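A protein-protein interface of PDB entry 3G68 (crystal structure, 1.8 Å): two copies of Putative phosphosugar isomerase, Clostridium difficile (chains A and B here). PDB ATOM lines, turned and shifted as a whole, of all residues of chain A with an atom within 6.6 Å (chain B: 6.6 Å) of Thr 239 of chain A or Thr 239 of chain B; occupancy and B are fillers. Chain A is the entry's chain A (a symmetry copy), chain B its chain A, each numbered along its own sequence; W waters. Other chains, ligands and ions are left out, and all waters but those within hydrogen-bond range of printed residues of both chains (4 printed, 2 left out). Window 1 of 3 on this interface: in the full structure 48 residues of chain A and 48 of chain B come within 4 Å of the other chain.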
ATOM      1  N   ILE A 211      25.958 -24.297   9.840  1.00  0.00           N
ATOM      2  CA  ILE A 211      25.749 -25.714   9.526  1.00  0.00           C
ATOM      3  C   ILE A 211      24.730 -25.915   8.418  1.00  0.00           C
ATOM      4  O   ILE A 211      23.764 -25.185   8.308  1.00  0.00           O
ATOM      5  CB  ILE A 211      25.220 -26.485  10.769  1.00  0.00           C
ATOM      6  CG1 ILE A 211      26.231 -26.352  11.936  1.00  0.00           C
ATOM      7  CG2 ILE A 211      24.882 -27.994  10.419  1.00  0.00           C
ATOM      8  CD1 ILE A 211      25.681 -26.664  13.357  1.00  0.00           C
ATOM      9  N   ARG A 212      24.978 -26.913   7.584  1.00  0.00           N
ATOM     10  CA  ARG A 212      23.978 -27.350   6.599  1.00  0.00           C
ATOM     11  C   ARG A 212      23.839 -28.859   6.734  1.00  0.00           C
ATOM     12  O   ARG A 212      24.807 -29.546   7.018  1.00  0.00           O
ATOM     13  CB  ARG A 212      24.333 -26.954   5.183  1.00  0.00           C
ATOM     14  CG  ARG A 212      24.337 -25.453   4.987  1.00  0.00           C
ATOM     15  CD  ARG A 212      24.642 -25.104   3.523  1.00  0.00           C
ATOM     16  NE  ARG A 212      24.574 -23.655   3.305  1.00  0.00           N
ATOM     17  CZ  ARG A 212      25.570 -22.792   3.486  1.00  0.00           C
ATOM     18  NH1 ARG A 212      26.775 -23.198   3.873  1.00  0.00           N
ATOM     19  NH2 ARG A 212      25.351 -21.505   3.250  1.00  0.00           N
ATOM     20  N   ILE A 213      22.621 -29.356   6.587  1.00  0.00           N
ATOM     21  CA  ILE A 213      22.330 -30.791   6.665  1.00  0.00           C
ATOM     22  C   ILE A 213      21.820 -31.223   5.302  1.00  0.00           C
ATOM     23  O   ILE A 213      20.985 -30.530   4.725  1.00  0.00           O
ATOM     24  CB  ILE A 213      21.282 -31.112   7.713  1.00  0.00           C
ATOM     25  CG1 ILE A 213      21.669 -30.445   9.036  1.00  0.00           C
ATOM     26  CG2 ILE A 213      21.116 -32.660   7.856  1.00  0.00           C
ATOM     27  CD1 ILE A 213      20.752 -30.794  10.169  1.00  0.00           C
ATOM     28  N   ILE A 214      22.351 -32.336   4.784  1.00  0.00           N
ATOM     29  CA  ILE A 214      21.947 -32.873   3.474  1.00  0.00           C
ATOM     30  C   ILE A 214      21.350 -34.252   3.703  1.00  0.00           C
ATOM     31  O   ILE A 214      22.048 -35.163   4.204  1.00  0.00           O
ATOM     32  CB  ILE A 214      23.170 -32.999   2.497  1.00  0.00           C
ATOM     33  CG1 ILE A 214      23.902 -31.657   2.364  1.00  0.00           C
ATOM     34  CG2 ILE A 214      22.717 -33.476   1.109  1.00  0.00           C
ATOM     35  CD1 ILE A 214      25.196 -31.781   1.413  1.00  0.00           C
ATOM     36  N   THR A 223      15.208 -33.915   8.109  1.00  0.00           N
ATOM     37  CA  THR A 223      16.320 -33.056   7.721  1.00  0.00           C
ATOM     38  C   THR A 223      15.966 -31.596   8.118  1.00  0.00           C
ATOM     39  O   THR A 223      16.765 -30.906   8.743  1.00  0.00           O
ATOM     40  CB  THR A 223      16.648 -33.209   6.230  1.00  0.00           C
ATOM     41  OG1 THR A 223      17.034 -34.575   5.992  1.00  0.00           O
ATOM     42  CG2 THR A 223      17.821 -32.312   5.779  1.00  0.00           C
ATOM     43  N   LEU A 224      14.752 -31.160   7.786  1.00  0.00           N
ATOM     44  CA  LEU A 224      14.304 -29.814   8.181  1.00  0.00           C
ATOM     45  C   LEU A 224      14.257 -29.630   9.702  1.00  0.00           C
ATOM     46  O   LEU A 224      14.638 -28.571  10.212  1.00  0.00           O
ATOM     47  CB  LEU A 224      12.943 -29.520   7.583  1.00  0.00           C
ATOM     48  CG  LEU A 224      12.834 -29.483   6.052  1.00  0.00           C
ATOM     49  CD1 LEU A 224      11.388 -29.206   5.679  1.00  0.00           C
ATOM     50  CD2 LEU A 224      13.804 -28.415   5.434  1.00  0.00           C
ATOM     51  N   ALA A 227      17.674 -29.334  11.340  1.00  0.00           N
ATOM     52  CA  ALA A 227      18.177 -28.002  11.066  1.00  0.00           C
ATOM     53  C   ALA A 227      17.575 -26.983  12.005  1.00  0.00           C
ATOM     54  O   ALA A 227      18.315 -26.199  12.634  1.00  0.00           O
ATOM     55  CB  ALA A 227      17.906 -27.605   9.582  1.00  0.00           C
ATOM     56  N   LEU A 228      16.246 -27.005  12.155  1.00  0.00           N
ATOM     57  CA  LEU A 228      15.578 -26.065  13.048  1.00  0.00           C
ATOM     58  C   LEU A 228      16.052 -26.210  14.498  1.00  0.00           C
ATOM     59  O   LEU A 228      16.288 -25.200  15.180  1.00  0.00           O
ATOM     60  CB  LEU A 228      14.050 -26.184  12.996  1.00  0.00           C
ATOM     61  CG  LEU A 228      13.276 -25.278  13.948  1.00  0.00           C
ATOM     62  CD1 LEU A 228      13.560 -23.747  13.674  1.00  0.00           C
ATOM     63  CD2 LEU A 228      11.782 -25.585  13.880  1.00  0.00           C
ATOM     64  N   LEU A 231      19.525 -24.824  14.872  1.00  0.00           N
ATOM     65  CA  LEU A 231      19.405 -23.360  14.838  1.00  0.00           C
ATOM     66  C   LEU A 231      19.006 -22.773  16.211  1.00  0.00           C
ATOM     67  O   LEU A 231      19.659 -21.855  16.720  1.00  0.00           O
ATOM     68  CB  LEU A 231      18.428 -22.926  13.733  1.00  0.00           C
ATOM     69  CG  LEU A 231      18.178 -21.425  13.525  1.00  0.00           C
ATOM     70  CD1 LEU A 231      17.722 -21.168  12.107  1.00  0.00           C
ATOM     71  CD2 LEU A 231      17.149 -20.888  14.545  1.00  0.00           C
ATOM     72  N   PRO A 237      23.466 -19.836  11.858  1.00  0.00           N
ATOM     73  CA  PRO A 237      22.714 -20.264  10.676  1.00  0.00           C
ATOM     74  C   PRO A 237      22.767 -21.774  10.469  1.00  0.00           C
ATOM     75  O   PRO A 237      23.844 -22.358  10.569  1.00  0.00           O
ATOM     76  CB  PRO A 237      23.430 -19.561   9.538  1.00  0.00           C
ATOM     77  CG  PRO A 237      24.116 -18.335  10.225  1.00  0.00           C
ATOM     78  CD  PRO A 237      24.560 -18.911  11.507  1.00  0.00           C
ATOM     79  N   VAL A 238      21.610 -22.371  10.241  1.00  0.00           N
ATOM     80  CA  VAL A 238      21.493 -23.794   9.984  1.00  0.00           C
ATOM     81  C   VAL A 238      20.348 -24.025   9.004  1.00  0.00           C
ATOM     82  O   VAL A 238      19.209 -23.567   9.250  1.00  0.00           O
ATOM     83  CB  VAL A 238      21.205 -24.629  11.248  1.00  0.00           C
ATOM     84  CG1 VAL A 238      21.396 -26.132  10.919  1.00  0.00           C
ATOM     85  CG2 VAL A 238      22.128 -24.254  12.452  1.00  0.00           C
ATOM     86  N   THR A 239      20.634 -24.729   7.916  1.00  0.00           N
ATOM     87  CA  THR A 239      19.620 -25.069   6.918  1.00  0.00           C
ATOM     88  C   THR A 239      19.740 -26.522   6.514  1.00  0.00           C
ATOM     89  O   THR A 239      20.848 -27.065   6.449  1.00  0.00           O
ATOM     90  CB  THR A 239      19.713 -24.152   5.650  1.00  0.00           C
ATOM     91  OG1 THR A 239      19.650 -22.790   6.057  1.00  0.00           O
ATOM     92  CG2 THR A 239      18.535 -24.430   4.603  1.00  0.00           C
ATOM     93  N   GLY A 240      18.576 -27.143   6.306  1.00  0.00           N
ATOM     94  CA  GLY A 240      18.416 -28.483   5.829  1.00  0.00           C
ATOM     95  C   GLY A 240      18.031 -28.518   4.345  1.00  0.00           C
ATOM     96  O   GLY A 240      17.221 -27.709   3.884  1.00  0.00           O
ATOM     97  N   TYR A 241      18.585 -29.473   3.605  1.00  0.00           N
ATOM     98  CA  TYR A 241      18.327 -29.613   2.178  1.00  0.00           C
ATOM     99  C   TYR A 241      18.219 -31.049   1.751  1.00  0.00           C
ATOM    100  O   TYR A 241      18.907 -31.909   2.321  1.00  0.00           O
ATOM    101  CB  TYR A 241      19.530 -29.073   1.377  1.00  0.00           C
ATOM    102  CG  TYR A 241      19.965 -27.686   1.686  1.00  0.00           C
ATOM    103  CD1 TYR A 241      20.863 -27.444   2.712  1.00  0.00           C
ATOM    104  CD2 TYR A 241      19.434 -26.596   0.990  1.00  0.00           C
ATOM    105  CE1 TYR A 241      21.264 -26.168   3.012  1.00  0.00           C
ATOM    106  CE2 TYR A 241      19.816 -25.318   1.298  1.00  0.00           C
ATOM    107  CZ  TYR A 241      20.772 -25.113   2.300  1.00  0.00           C
ATOM    108  OH  TYR A 241      21.169 -23.820   2.601  1.00  0.00           O
ATOM    109  N   ILE B 211      22.554 -13.745   6.146  1.00  0.00           N
ATOM    110  CA  ILE B 211      21.322 -13.002   5.862  1.00  0.00           C
ATOM    111  C   ILE B 211      20.079 -13.859   6.031  1.00  0.00           C
ATOM    112  O   ILE B 211      20.082 -15.040   5.741  1.00  0.00           O
ATOM    113  CB  ILE B 211      21.315 -12.482   4.396  1.00  0.00           C
ATOM    114  CG1 ILE B 211      22.542 -11.568   4.159  1.00  0.00           C
ATOM    115  CG2 ILE B 211      19.942 -11.773   4.036  1.00  0.00           C
ATOM    116  CD1 ILE B 211      22.940 -11.327   2.675  1.00  0.00           C
ATOM    117  N   ARG B 212      19.019 -13.242   6.528  1.00  0.00           N
ATOM    118  CA  ARG B 212      17.701 -13.889   6.550  1.00  0.00           C
ATOM    119  C   ARG B 212      16.704 -12.912   5.944  1.00  0.00           C
ATOM    120  O   ARG B 212      16.836 -11.710   6.116  1.00  0.00           O
ATOM    121  CB  ARG B 212      17.276 -14.318   7.938  1.00  0.00           C
ATOM    122  CG  ARG B 212      18.171 -15.398   8.507  1.00  0.00           C
ATOM    123  CD  ARG B 212      17.664 -15.841   9.887  1.00  0.00           C
ATOM    124  NE  ARG B 212      18.480 -16.941  10.415  1.00  0.00           N
ATOM    125  CZ  ARG B 212      19.604 -16.812  11.114  1.00  0.00           C
ATOM    126  NH1 ARG B 212      20.089 -15.615  11.429  1.00  0.00           N
ATOM    127  NH2 ARG B 212      20.233 -17.907  11.521  1.00  0.00           N
ATOM    128  N   ILE B 213      15.750 -13.431   5.188  1.00  0.00           N
ATOM    129  CA  ILE B 213      14.704 -12.622   4.555  1.00  0.00           C
ATOM    130  C   ILE B 213      13.377 -13.049   5.155  1.00  0.00           C
ATOM    131  O   ILE B 213      13.133 -14.247   5.284  1.00  0.00           O
ATOM    132  CB  ILE B 213      14.656 -12.814   3.052  1.00  0.00           C
ATOM    133  CG1 ILE B 213      16.063 -12.641   2.474  1.00  0.00           C
ATOM    134  CG2 ILE B 213      13.627 -11.825   2.413  1.00  0.00           C
ATOM    135  CD1 ILE B 213      16.103 -12.702   0.977  1.00  0.00           C
ATOM    136  N   ILE B 214      12.551 -12.074   5.551  1.00  0.00           N
ATOM    137  CA  ILE B 214      11.232 -12.343   6.145  1.00  0.00           C
ATOM    138  C   ILE B 214      10.180 -11.737   5.231  1.00  0.00           C
ATOM    139  O   ILE B 214      10.172 -10.503   5.017  1.00  0.00           O
ATOM    140  CB  ILE B 214      11.098 -11.708   7.574  1.00  0.00           C
ATOM    141  CG1 ILE B 214      12.242 -12.173   8.486  1.00  0.00           C
ATOM    142  CG2 ILE B 214       9.751 -12.074   8.215  1.00  0.00           C
ATOM    143  CD1 ILE B 214      12.156 -11.483   9.939  1.00  0.00           C
ATOM    144  N   THR B 223      10.350 -14.867  -1.655  1.00  0.00           N
ATOM    145  CA  THR B 223      11.182 -14.817  -0.459  1.00  0.00           C
ATOM    146  C   THR B 223      12.247 -15.945  -0.561  1.00  0.00           C
ATOM    147  O   THR B 223      13.433 -15.705  -0.362  1.00  0.00           O
ATOM    148  CB  THR B 223      10.333 -14.908   0.815  1.00  0.00           C
ATOM    149  OG1 THR B 223       9.441 -13.778   0.843  1.00  0.00           O
ATOM    150  CG2 THR B 223      11.180 -14.859   2.105  1.00  0.00           C
ATOM    151  N   LEU B 224      11.811 -17.152  -0.915  1.00  0.00           N
ATOM    152  CA  LEU B 224      12.756 -18.266  -1.103  1.00  0.00           C
ATOM    153  C   LEU B 224      13.767 -17.999  -2.224  1.00  0.00           C
ATOM    154  O   LEU B 224      14.950 -18.326  -2.084  1.00  0.00           O
ATOM    155  CB  LEU B 224      12.002 -19.550  -1.384  1.00  0.00           C
ATOM    156  CG  LEU B 224      11.065 -20.077  -0.287  1.00  0.00           C
ATOM    157  CD1 LEU B 224      10.396 -21.343  -0.792  1.00  0.00           C
ATOM    158  CD2 LEU B 224      11.839 -20.328   1.055  1.00  0.00           C
ATOM    159  N   ALA B 227      16.438 -15.447  -1.333  1.00  0.00           N
ATOM    160  CA  ALA B 227      17.391 -16.097  -0.455  1.00  0.00           C
ATOM    161  C   ALA B 227      18.373 -16.938  -1.236  1.00  0.00           C
ATOM    162  O   ALA B 227      19.600 -16.802  -1.049  1.00  0.00           O
ATOM    163  CB  ALA B 227      16.653 -16.965   0.610  1.00  0.00           C
ATOM    164  N   LEU B 228      17.866 -17.775  -2.148  1.00  0.00           N
ATOM    165  CA  LEU B 228      18.740 -18.619  -2.956  1.00  0.00           C
ATOM    166  C   LEU B 228      19.715 -17.795  -3.805  1.00  0.00           C
ATOM    167  O   LEU B 228      20.905 -18.139  -3.894  1.00  0.00           O
ATOM    168  CB  LEU B 228      17.961 -19.580  -3.862  1.00  0.00           C
ATOM    169  CG  LEU B 228      18.800 -20.455  -4.787  1.00  0.00           C
ATOM    170  CD1 LEU B 228      19.790 -21.389  -3.984  1.00  0.00           C
ATOM    171  CD2 LEU B 228      17.899 -21.268  -5.713  1.00  0.00           C
ATOM    172  N   LEU B 231      22.390 -16.305  -1.625  1.00  0.00           N
ATOM    173  CA  LEU B 231      23.301 -17.398  -1.262  1.00  0.00           C
ATOM    174  C   LEU B 231      24.341 -17.685  -2.369  1.00  0.00           C
ATOM    175  O   LEU B 231      25.548 -17.734  -2.106  1.00  0.00           O
ATOM    176  CB  LEU B 231      22.506 -18.661  -0.893  1.00  0.00           C
ATOM    177  CG  LEU B 231      23.283 -19.917  -0.466  1.00  0.00           C
ATOM    178  CD1 LEU B 231      22.409 -20.796   0.400  1.00  0.00           C
ATOM    179  CD2 LEU B 231      23.802 -20.691  -1.698  1.00  0.00           C
ATOM    180  N   PRO B 237      25.669 -17.914   4.387  1.00  0.00           N
ATOM    181  CA  PRO B 237      24.347 -18.457   4.708  1.00  0.00           C
ATOM    182  C   PRO B 237      23.231 -17.445   4.474  1.00  0.00           C
ATOM    183  O   PRO B 237      23.369 -16.291   4.878  1.00  0.00           O
ATOM    184  CB  PRO B 237      24.453 -18.775   6.187  1.00  0.00           C
ATOM    185  CG  PRO B 237      25.988 -18.962   6.423  1.00  0.00           C
ATOM    186  CD  PRO B 237      26.560 -17.910   5.563  1.00  0.00           C
ATOM    187  N   VAL B 238      22.187 -17.877   3.787  1.00  0.00           N
ATOM    188  CA  VAL B 238      21.025 -17.052   3.513  1.00  0.00           C
ATOM    189  C   VAL B 238      19.785 -17.938   3.503  1.00  0.00           C
ATOM    190  O   VAL B 238      19.741 -18.950   2.766  1.00  0.00           O
ATOM    191  CB  VAL B 238      21.092 -16.321   2.158  1.00  0.00           C
ATOM    192  CG1 VAL B 238      19.968 -15.254   2.099  1.00  0.00           C
ATOM    193  CG2 VAL B 238      22.467 -15.621   1.908  1.00  0.00           C
ATOM    194  N   THR B 239      18.786 -17.567   4.296  1.00  0.00           N
ATOM    195  CA  THR B 239      17.519 -18.295   4.346  1.00  0.00           C
ATOM    196  C   THR B 239      16.352 -17.331   4.315  1.00  0.00           C
ATOM    197  O   THR B 239      16.433 -16.232   4.874  1.00  0.00           O
ATOM    198  CB  THR B 239      17.419 -19.215   5.610  1.00  0.00           C
ATOM    199  OG1 THR B 239      18.550 -20.077   5.647  1.00  0.00           O
ATOM    200  CG2 THR B 239      16.092 -20.109   5.618  1.00  0.00           C
ATOM    201  N   GLY B 240      15.302 -17.747   3.604  1.00  0.00           N
ATOM    202  CA  GLY B 240      14.046 -17.069   3.493  1.00  0.00           C
ATOM    203  C   GLY B 240      12.968 -17.719   4.369  1.00  0.00           C
ATOM    204  O   GLY B 240      12.883 -18.947   4.458  1.00  0.00           O
ATOM    205  N   TYR B 241      12.126 -16.898   4.989  1.00  0.00           N
ATOM    206  CA  TYR B 241      11.068 -17.375   5.870  1.00  0.00           C
ATOM    207  C   TYR B 241       9.799 -16.583   5.725  1.00  0.00           C
ATOM    208  O   TYR B 241       9.862 -15.371   5.467  1.00  0.00           O
ATOM    209  CB  TYR B 241      11.478 -17.159   7.341  1.00  0.00           C
ATOM    210  CG  TYR B 241      12.786 -17.731   7.755  1.00  0.00           C
ATOM    211  CD1 TYR B 241      13.954 -17.007   7.587  1.00  0.00           C
ATOM    212  CD2 TYR B 241      12.871 -19.030   8.266  1.00  0.00           C
ATOM    213  CE1 TYR B 241      15.167 -17.527   7.958  1.00  0.00           C
ATOM    214  CE2 TYR B 241      14.082 -19.563   8.620  1.00  0.00           C
ATOM    215  CZ  TYR B 241      15.236 -18.780   8.494  1.00  0.00           C
ATOM    216  OH  TYR B 241      16.459 -19.315   8.866  1.00  0.00           O
HETATM  217  O   HOH W   1      19.601 -21.972   1.992  1.00  0.00           O
HETATM  218  O   HOH W   2      19.365 -20.052   9.600  1.00  0.00           O
HETATM  219  O   HOH W   3      16.652 -21.806   8.904  1.00  0.00           O
HETATM  220  O   HOH W   4      22.382 -21.156   3.578  1.00  0.00           O
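Among the printed residues, merely in contact across the chains: Arg 212 of chain A with Pro 237 of chain B (3.5 Å), Pro 237 of chain A with Arg 212 of chain B (3.5 Å), Pro 237 of chain A with Pro 237 of chain B (3.6 Å), Tyr 241 of chain A with Leu 231 of chain B (3.9 Å) and Leu 231 of chain A with Tyr 241 of chain B (3.9 Å).
Printed residues of chain A that touch a printed residue of chain B: Arg 212, Leu 231, Pro 237, Thr 239 and Tyr 241. Of the 14 printed residues of chain B, 5 touch a printed residue of chain A. Hydrophobic or aromatic side chains of chain B that line the printed part of chain A: Leu 231, Pro 237 and Tyr 241.
Water W3 bridges OH of Tyr 241 of chain B (2.5 Å) and O of Val 238 of chain A (3.1 Å). Water W1 bridges the side-chain hydroxyl of Tyr 241 of chain A (2.5 Å) and the backbone carbonyl oxygen of Val 238 of chain B (3.1 Å). Water W4 lies within hydrogen-bond range of the guanidinium group (NH2) of Arg 212 of chain A, the side-chain hydroxyl (OH) of Tyr 241 of chain A and the backbone NH (N) of Val 238 of chain B. Water W2 lies within hydrogen-bond range of NH2 of Arg 212 of chain B (3.0 Å), OH of Tyr 241 of chain B (3.1 Å) and N of Val 238 of chain A (3.3 Å).
N of Ile 211 of chain B sits at hydrogen-bond distance from O of Pro 237 of chain B, 3.0 Å away. N of Thr 239 of chain B sits at hydrogen-bond distance from O of Ile 211 of chain B, 3.2 Å away. NE of Arg 212 of chain B is in hydrogen-bond range of OH of Tyr 241 of chain B. O of Ile 211 of chain A sits at hydrogen-bond distance from N of Thr 239 of chain A, 3.2 Å away. OH of Tyr 241 of chain A sits at hydrogen-bond distance from NE of Arg 212 of chain A (3.5 Å). O of Ile 213 of chain A sits at hydrogen-bond distance from N of Tyr 241 of chain A (2.9 Å).
OG1 of Thr 239 of chain A sits at hydrogen-bond distance from OG1 of Thr 239 of chain B (3.0 Å).
Of chain B, only Thr 239 comes within 4 Å of Thr 239 of chain A. Ile 213 of chain B touches none of the printed residues of chain A. Of the printed residues of chain A, Pro 237 of chain B touches Arg 212 and Pro 237. Of chain A, only Thr 239 comes within 4 Å of Thr 239 of chain B. Of the printed residues of chain A, Tyr 241 of chain B touches Leu 231. The nearest printed residue of chain A that does not touch Tyr 241 of chain B is Val 238 of chain A (5.1 Å).
Arg 212 of chain A touches Pro 237 of chain B, and with the chains exchanged Pro 237 of chain A touches Arg 212 of chain B. Leu 231 of chain A touches Tyr 241 of chain B, and with the chains exchanged Tyr 241 of chain A touches Leu 231 of chain B. Pro 237 of chain A touches its own counterpart, Pro 237 of chain B. Thr 239 of chain A touches its own counterpart, Thr 239 of chain B. Of the 6 pairs that touch across the chains among the printed residues, 6 have their exchanged pair printed and touching as well.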
